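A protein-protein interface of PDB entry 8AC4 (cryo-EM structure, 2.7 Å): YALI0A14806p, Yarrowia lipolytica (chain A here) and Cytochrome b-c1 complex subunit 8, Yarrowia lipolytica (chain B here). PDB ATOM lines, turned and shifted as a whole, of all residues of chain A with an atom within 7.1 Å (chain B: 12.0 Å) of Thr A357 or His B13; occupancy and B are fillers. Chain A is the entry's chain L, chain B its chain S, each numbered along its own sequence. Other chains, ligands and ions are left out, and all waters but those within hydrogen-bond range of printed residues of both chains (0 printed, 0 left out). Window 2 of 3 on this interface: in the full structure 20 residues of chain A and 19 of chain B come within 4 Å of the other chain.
The side-chain carboxylate (OE2) of Glu A457 is in hydrogen-bond range of the backbone NH (N) of Gly B12, 2.9 Å away. OE2 of Glu A457 lies within hydrogen-bond range of N of His B13, 2.9 Å away. The backbone NH of Met B14 sits at hydrogen-bond distance from the side-chain carboxylate of Glu A457 (2.6 Å). The backbone carbonyl oxygen (O) of Trp B10 sits close to the side-chain carboxylate (OE2) of Glu A457.
The side-chain amide oxygen (OD1) of Asn A355 is in hydrogen-bond range of the side-chain hydroxyl (OG1) of Thr A357 (3.5 Å). The backbone NH (N) of Gly B9 sits at hydrogen-bond distance from the backbone carbonyl oxygen (O) of Met B14 (2.9 Å).
O of Thr A356 touches CA of Gly B12, 3.8 Å away. ND1 of His B13 touches CG2 of Thr A357, at 3.9 Å. Trp B11 touches Glu A457. CA of Gly A458 touches N of Gly B12, 3.9 Å away.
Of the 13 printed residues of chain B, 5 touch a printed residue of chain A. Hydrophobic or aromatic side chains of chain B that line the printed part of chain A: Trp B11, His B13 and Met B14. Printed residues of chain A that touch a printed residue of chain B: Thr A356, Thr A357, Glu A457 and Gly A458. Among the printed residues, no Asp or Glu carboxylate lies within 4 Å of a Lys or Arg side-chain nitrogen of the other chain.
Thr A357 touches just one residue of chain B: His B13 (3.9 Å). Printed residues of chain A within 4 Å of His B13: Thr A357 and Glu A457. Asn A355 touches none of the printed residues of chain B. No residue of chain B comes within 4 Å of Gln A358. No residue of chain B comes within 4 Å of Ile A359. No residue of chain B comes within 4 Å of Asp A360. Printed residues of chain B within 4 Å of Gly A458: Gly B12 (3.9 Å). Printed residues of chain A within 4 Å of Met B14: Glu A457. Of the printed residues of chain A, Trp B10 touches Glu A457 (3.5 Å). Gln B19 touches none of the printed residues of chain A. Gly B9 touches none of the printed residues of chain A. The nearest residue of chain B that does not touch Thr A357 is Trp B11 (4.3 Å). The nearest residue of chain A that does not touch His B13 is Thr A356 (6.0 Å).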
ATOM      1  N   SER A 353      15.953   0.030   5.299  1.00  0.00           N
ATOM      2  CA  SER A 353      15.325  -1.254   5.077  1.00  0.00           C
ATOM      3  C   SER A 353      15.935  -1.898   3.845  1.00  0.00           C
ATOM      4  O   SER A 353      16.124  -1.229   2.832  1.00  0.00           O
ATOM      5  CB  SER A 353      13.844  -1.070   4.897  1.00  0.00           C
ATOM      6  OG  SER A 353      13.220  -2.291   4.531  1.00  0.00           O
ATOM      7  N   GLU A 354      16.155  -3.214   3.930  1.00  0.00           N
ATOM      8  CA  GLU A 354      16.504  -4.012   2.765  1.00  0.00           C
ATOM      9  C   GLU A 354      15.278  -4.740   2.222  1.00  0.00           C
ATOM     10  O   GLU A 354      15.369  -5.452   1.228  1.00  0.00           O
ATOM     11  CB  GLU A 354      17.509  -5.094   3.144  1.00  0.00           C
ATOM     12  CG  GLU A 354      18.880  -4.563   3.519  1.00  0.00           C
ATOM     13  CD  GLU A 354      19.689  -5.403   4.506  1.00  0.00           C
ATOM     14  OE1 GLU A 354      20.878  -5.069   4.745  1.00  0.00           O
ATOM     15  OE2 GLU A 354      19.136  -6.389   5.056  1.00  0.00           O
ATOM     16  N   ASN A 355      14.146  -4.625   2.909  1.00  0.00           N
ATOM     17  CA  ASN A 355      12.984  -5.400   2.528  1.00  0.00           C
ATOM     18  C   ASN A 355      12.247  -4.603   1.468  1.00  0.00           C
ATOM     19  O   ASN A 355      11.287  -3.905   1.766  1.00  0.00           O
ATOM     20  CB  ASN A 355      12.112  -5.693   3.748  1.00  0.00           C
ATOM     21  CG  ASN A 355      10.967  -6.663   3.525  1.00  0.00           C
ATOM     22  OD1 ASN A 355      10.597  -6.985   2.395  1.00  0.00           O
ATOM     23  ND2 ASN A 355      10.394  -7.145   4.617  1.00  0.00           N
ATOM     24  N   THR A 356      12.679  -4.733   0.225  1.00  0.00           N
ATOM     25  CA  THR A 356      12.241  -3.758  -0.755  1.00  0.00           C
ATOM     26  C   THR A 356      10.824  -4.021  -1.254  1.00  0.00           C
ATOM     27  O   THR A 356      10.213  -3.135  -1.839  1.00  0.00           O
ATOM     28  CB  THR A 356      13.262  -3.643  -1.878  1.00  0.00           C
ATOM     29  OG1 THR A 356      13.426  -4.969  -2.375  1.00  0.00           O
ATOM     30  CG2 THR A 356      14.568  -3.075  -1.373  1.00  0.00           C
ATOM     31  N   THR A 357      10.295  -5.211  -0.989  1.00  0.00           N
ATOM     32  CA  THR A 357       8.930  -5.505  -1.381  1.00  0.00           C
ATOM     33  C   THR A 357       7.941  -5.185  -0.264  1.00  0.00           C
ATOM     34  O   THR A 357       6.738  -5.345  -0.451  1.00  0.00           O
ATOM     35  CB  THR A 357       8.813  -6.957  -1.838  1.00  0.00           C
ATOM     36  OG1 THR A 357       9.122  -7.743  -0.687  1.00  0.00           O
ATOM     37  CG2 THR A 357       9.761  -7.263  -2.975  1.00  0.00           C
ATOM     38  N   GLN A 358       8.417  -4.750   0.903  1.00  0.00           N
ATOM     39  CA  GLN A 358       7.447  -4.433   1.938  1.00  0.00           C
ATOM     40  C   GLN A 358       7.687  -3.043   2.501  1.00  0.00           C
ATOM     41  O   GLN A 358       7.301  -2.744   3.632  1.00  0.00           O
ATOM     42  CB  GLN A 358       7.481  -5.483   3.028  1.00  0.00           C
ATOM     43  CG  GLN A 358       6.843  -6.794   2.631  1.00  0.00           C
ATOM     44  CD  GLN A 358       6.749  -7.589   3.904  1.00  0.00           C
ATOM     45  OE1 GLN A 358       7.642  -8.375   4.224  1.00  0.00           O
ATOM     46  NE2 GLN A 358       5.700  -7.326   4.676  1.00  0.00           N
ATOM     47  N   ILE A 359       8.262  -2.180   1.668  1.00  0.00           N
ATOM     48  CA  ILE A 359       8.455  -0.795   2.045  1.00  0.00           C
ATOM     49  C   ILE A 359       7.097  -0.167   2.335  1.00  0.00           C
ATOM     50  O   ILE A 359       6.963   0.644   3.252  1.00  0.00           O
ATOM     51  CB  ILE A 359       9.225  -0.055   0.946  1.00  0.00           C
ATOM     52  CG1 ILE A 359      10.718  -0.324   1.088  1.00  0.00           C
ATOM     53  CG2 ILE A 359       8.942   1.435   0.968  1.00  0.00           C
ATOM     54  CD1 ILE A 359      11.465   0.148  -0.100  1.00  0.00           C
ATOM     55  N   ASP A 360       6.099  -0.567   1.546  1.00  0.00           N
ATOM     56  CA  ASP A 360       4.761  -0.039   1.712  1.00  0.00           C
ATOM     57  C   ASP A 360       4.268  -0.340   3.120  1.00  0.00           C
ATOM     58  O   ASP A 360       3.725   0.556   3.757  1.00  0.00           O
ATOM     59  CB  ASP A 360       3.805  -0.535   0.633  1.00  0.00           C
ATOM     60  CG  ASP A 360       3.586  -2.037   0.607  1.00  0.00           C
ATOM     61  OD1 ASP A 360       4.532  -2.785   0.943  1.00  0.00           O
ATOM     62  OD2 ASP A 360       2.467  -2.449   0.227  1.00  0.00           O
ATOM     63  N   ASP A 361       4.508  -1.568   3.606  1.00  0.00           N
ATOM     64  CA  ASP A 361       4.062  -1.957   4.934  1.00  0.00           C
ATOM     65  C   ASP A 361       4.816  -1.157   5.984  1.00  0.00           C
ATOM     66  O   ASP A 361       4.209  -0.648   6.921  1.00  0.00           O
ATOM     67  CB  ASP A 361       4.213  -3.454   5.184  1.00  0.00           C
ATOM     68  CG  ASP A 361       3.317  -4.290   4.290  1.00  0.00           C
ATOM     69  OD1 ASP A 361       2.113  -3.967   4.186  1.00  0.00           O
ATOM     70  OD2 ASP A 361       3.833  -5.248   3.690  1.00  0.00           O
ATOM     71  N   PRO A 455      16.539   1.698  -3.436  1.00  0.00           N
ATOM     72  CA  PRO A 455      15.534   0.923  -4.158  1.00  0.00           C
ATOM     73  C   PRO A 455      14.128   1.141  -3.606  1.00  0.00           C
ATOM     74  O   PRO A 455      13.615   0.320  -2.856  1.00  0.00           O
ATOM     75  CB  PRO A 455      16.083  -0.476  -3.914  1.00  0.00           C
ATOM     76  CG  PRO A 455      16.608  -0.398  -2.502  1.00  0.00           C
ATOM     77  CD  PRO A 455      17.354   0.910  -2.499  1.00  0.00           C
ATOM     78  N   GLU A 457      11.238   1.720  -5.382  1.00  0.00           N
ATOM     79  CA  GLU A 457      10.135   1.431  -6.292  1.00  0.00           C
ATOM     80  C   GLU A 457       8.851   1.135  -5.515  1.00  0.00           C
ATOM     81  O   GLU A 457       7.768   1.537  -5.930  1.00  0.00           O
ATOM     82  CB  GLU A 457      10.446   0.226  -7.176  1.00  0.00           C
ATOM     83  CG  GLU A 457       9.346  -0.063  -8.178  1.00  0.00           C
ATOM     84  CD  GLU A 457       9.602  -1.285  -9.035  1.00  0.00           C
ATOM     85  OE1 GLU A 457      10.301  -1.161 -10.065  1.00  0.00           O
ATOM     86  OE2 GLU A 457       9.109  -2.362  -8.660  1.00  0.00           O
ATOM     87  N   GLY A 458       8.984   0.436  -4.384  1.00  0.00           N
ATOM     88  CA  GLY A 458       7.834   0.042  -3.593  1.00  0.00           C
ATOM     89  C   GLY A 458       7.249   1.165  -2.740  1.00  0.00           C
ATOM     90  O   GLY A 458       6.253   0.955  -2.057  1.00  0.00           O
ATOM     91  N   TYR B   7       5.590 -10.134 -17.622  1.00  0.00           N
ATOM     92  CA  TYR B   7       6.036  -8.775 -18.236  1.00  0.00           C
ATOM     93  C   TYR B   7       5.711  -7.572 -17.345  1.00  0.00           C
ATOM     94  O   TYR B   7       6.183  -6.449 -17.570  1.00  0.00           O
ATOM     95  CB  TYR B   7       5.434  -8.521 -19.625  1.00  0.00           C
ATOM     96  CG  TYR B   7       6.025  -9.351 -20.737  1.00  0.00           C
ATOM     97  CD1 TYR B   7       7.363  -9.241 -21.094  1.00  0.00           C
ATOM     98  CD2 TYR B   7       5.248 -10.288 -21.403  1.00  0.00           C
ATOM     99  CE1 TYR B   7       7.915 -10.042 -22.085  1.00  0.00           C
ATOM    100  CE2 TYR B   7       5.783 -11.087 -22.402  1.00  0.00           C
ATOM    101  CZ  TYR B   7       7.119 -10.963 -22.747  1.00  0.00           C
ATOM    102  OH  TYR B   7       7.642 -11.749 -23.737  1.00  0.00           O
ATOM    103  N   MET B   8       4.839  -7.778 -16.365  1.00  0.00           N
ATOM    104  CA  MET B   8       4.696  -6.789 -15.319  1.00  0.00           C
ATOM    105  C   MET B   8       4.879  -7.501 -13.989  1.00  0.00           C
ATOM    106  O   MET B   8       4.345  -8.593 -13.797  1.00  0.00           O
ATOM    107  CB  MET B   8       3.328  -6.120 -15.379  1.00  0.00           C
ATOM    108  CG  MET B   8       3.199  -5.051 -14.328  1.00  0.00           C
ATOM    109  SD  MET B   8       1.550  -4.365 -14.245  1.00  0.00           S
ATOM    110  CE  MET B   8       0.600  -5.750 -13.617  1.00  0.00           C
ATOM    111  N   GLY B   9       5.628  -6.883 -13.074  1.00  0.00           N
ATOM    112  CA  GLY B   9       5.733  -7.491 -11.764  1.00  0.00           C
ATOM    113  C   GLY B   9       4.746  -6.859 -10.796  1.00  0.00           C
ATOM    114  O   GLY B   9       3.541  -6.793 -11.040  1.00  0.00           O
ATOM    115  N   TRP B  10       5.290  -6.404  -9.677  1.00  0.00           N
ATOM    116  CA  TRP B  10       4.494  -5.791  -8.638  1.00  0.00           C
ATOM    117  C   TRP B  10       5.390  -4.784  -7.940  1.00  0.00           C
ATOM    118  O   TRP B  10       6.570  -4.703  -8.250  1.00  0.00           O
ATOM    119  CB  TRP B  10       3.966  -6.852  -7.673  1.00  0.00           C
ATOM    120  CG  TRP B  10       2.736  -6.380  -6.963  1.00  0.00           C
ATOM    121  CD1 TRP B  10       2.624  -5.964  -5.665  1.00  0.00           C
ATOM    122  CD2 TRP B  10       1.435  -6.213  -7.557  1.00  0.00           C
ATOM    123  NE1 TRP B  10       1.334  -5.572  -5.405  1.00  0.00           N
ATOM    124  CE2 TRP B  10       0.580  -5.714  -6.546  1.00  0.00           C
ATOM    125  CE3 TRP B  10       0.919  -6.438  -8.844  1.00  0.00           C
ATOM    126  CZ2 TRP B  10      -0.774  -5.454  -6.785  1.00  0.00           C
ATOM    127  CZ3 TRP B  10      -0.422  -6.195  -9.073  1.00  0.00           C
ATOM    128  CH2 TRP B  10      -1.254  -5.706  -8.056  1.00  0.00           C
ATOM    129  N   TRP B  11       4.821  -3.981  -7.052  1.00  0.00           N
ATOM    130  CA  TRP B  11       5.614  -2.958  -6.402  1.00  0.00           C
ATOM    131  C   TRP B  11       6.843  -3.576  -5.756  1.00  0.00           C
ATOM    132  O   TRP B  11       6.737  -4.547  -5.008  1.00  0.00           O
ATOM    133  CB  TRP B  11       4.761  -2.320  -5.330  1.00  0.00           C
ATOM    134  CG  TRP B  11       3.521  -1.744  -5.910  1.00  0.00           C
ATOM    135  CD1 TRP B  11       2.263  -2.267  -5.865  1.00  0.00           C
ATOM    136  CD2 TRP B  11       3.439  -0.521  -6.652  1.00  0.00           C
ATOM    137  NE1 TRP B  11       1.396  -1.431  -6.511  1.00  0.00           N
ATOM    138  CE2 TRP B  11       2.083  -0.356  -7.006  1.00  0.00           C
ATOM    139  CE3 TRP B  11       4.376   0.440  -7.051  1.00  0.00           C
ATOM    140  CZ2 TRP B  11       1.641   0.737  -7.747  1.00  0.00           C
ATOM    141  CZ3 TRP B  11       3.937   1.527  -7.775  1.00  0.00           C
ATOM    142  CH2 TRP B  11       2.589   1.665  -8.122  1.00  0.00           C
ATOM    143  N   GLY B  12       7.998  -2.978  -6.029  1.00  0.00           N
ATOM    144  CA  GLY B  12       9.233  -3.539  -5.528  1.00  0.00           C
ATOM    145  C   GLY B  12       9.976  -4.336  -6.592  1.00  0.00           C
ATOM    146  O   GLY B  12      11.203  -4.361  -6.573  1.00  0.00           O
ATOM    147  N   HIS B  13       9.245  -4.972  -7.514  1.00  0.00           N
ATOM    148  CA  HIS B  13       9.888  -5.739  -8.567  1.00  0.00           C
ATOM    149  C   HIS B  13       9.073  -5.616  -9.851  1.00  0.00           C
ATOM    150  O   HIS B  13       8.658  -6.612 -10.441  1.00  0.00           O
ATOM    151  CB  HIS B  13      10.129  -7.178  -8.082  1.00  0.00           C
ATOM    152  CG  HIS B  13       8.866  -7.874  -7.707  1.00  0.00           C
ATOM    153  ND1 HIS B  13       8.206  -7.622  -6.520  1.00  0.00           N
ATOM    154  CD2 HIS B  13       8.122  -8.784  -8.375  1.00  0.00           C
ATOM    155  CE1 HIS B  13       7.115  -8.358  -6.463  1.00  0.00           C
ATOM    156  NE2 HIS B  13       7.035  -9.076  -7.595  1.00  0.00           N
ATOM    157  N   MET B  14       8.863  -4.376 -10.289  1.00  0.00           N
ATOM    158  CA  MET B  14       7.919  -4.106 -11.355  1.00  0.00           C
ATOM    159  C   MET B  14       8.452  -4.606 -12.697  1.00  0.00           C
ATOM    160  O   MET B  14       7.666  -4.936 -13.574  1.00  0.00           O
ATOM    161  CB  MET B  14       7.639  -2.608 -11.466  1.00  0.00           C
ATOM    162  CG  MET B  14       6.377  -2.285 -12.237  1.00  0.00           C
ATOM    163  SD  MET B  14       4.911  -2.773 -11.296  1.00  0.00           S
ATOM    164  CE  MET B  14       5.108  -1.707  -9.871  1.00  0.00           C
ATOM    165  N   GLY B  15       9.773  -4.677 -12.856  1.00  0.00           N
ATOM    166  CA  GLY B  15      10.332  -5.118 -14.123  1.00  0.00           C
ATOM    167  C   GLY B  15      10.903  -3.956 -14.934  1.00  0.00           C
ATOM    168  O   GLY B  15      11.155  -4.085 -16.132  1.00  0.00           O
ATOM    169  N   SER B  16      11.143  -2.833 -14.254  1.00  0.00           N
ATOM    170  CA  SER B  16      11.902  -1.731 -14.818  1.00  0.00           C
ATOM    171  C   SER B  16      13.346  -2.174 -15.044  1.00  0.00           C
ATOM    172  O   SER B  16      13.885  -2.979 -14.281  1.00  0.00           O
ATOM    173  CB  SER B  16      11.823  -0.542 -13.892  1.00  0.00           C
ATOM    174  OG  SER B  16      12.663   0.521 -14.318  1.00  0.00           O
ATOM    175  N   PRO B  17      14.036  -1.664 -16.088  1.00  0.00           N
ATOM    176  CA  PRO B  17      15.495  -1.746 -16.123  1.00  0.00           C
ATOM    177  C   PRO B  17      15.974  -0.971 -14.902  1.00  0.00           C
ATOM    178  O   PRO B  17      15.245  -0.130 -14.391  1.00  0.00           O
ATOM    179  CB  PRO B  17      15.848  -0.954 -17.375  1.00  0.00           C
ATOM    180  CG  PRO B  17      14.616  -1.065 -18.232  1.00  0.00           C
ATOM    181  CD  PRO B  17      13.462  -0.988 -17.261  1.00  0.00           C
ATOM    182  N   PRO B  18      17.180  -1.236 -14.362  1.00  0.00           N
ATOM    183  CA  PRO B  18      17.651  -0.505 -13.184  1.00  0.00           C
ATOM    184  C   PRO B  18      17.618   1.001 -13.420  1.00  0.00           C
ATOM    185  O   PRO B  18      18.018   1.479 -14.478  1.00  0.00           O
ATOM    186  CB  PRO B  18      19.096  -0.988 -13.058  1.00  0.00           C
ATOM    187  CG  PRO B  18      19.048  -2.376 -13.642  1.00  0.00           C
ATOM    188  CD  PRO B  18      18.140  -2.240 -14.843  1.00  0.00           C
ATOM    189  N   GLN B  19      17.079   1.728 -12.445  1.00  0.00           N
ATOM    190  CA  GLN B  19      17.032   3.174 -12.532  1.00  0.00           C
ATOM    191  C   GLN B  19      18.117   3.740 -11.636  1.00  0.00           C
ATOM    192  O   GLN B  19      18.340   3.245 -10.535  1.00  0.00           O
ATOM    193  CB  GLN B  19      15.686   3.686 -12.060  1.00  0.00           C
ATOM    194  CG  GLN B  19      14.556   3.022 -12.804  1.00  0.00           C
ATOM    195  CD  GLN B  19      13.270   3.776 -12.612  1.00  0.00           C
ATOM    196  OE1 GLN B  19      13.247   4.886 -12.072  1.00  0.00           O
ATOM    197  NE2 GLN B  19      12.184   3.161 -13.055  1.00  0.00           N
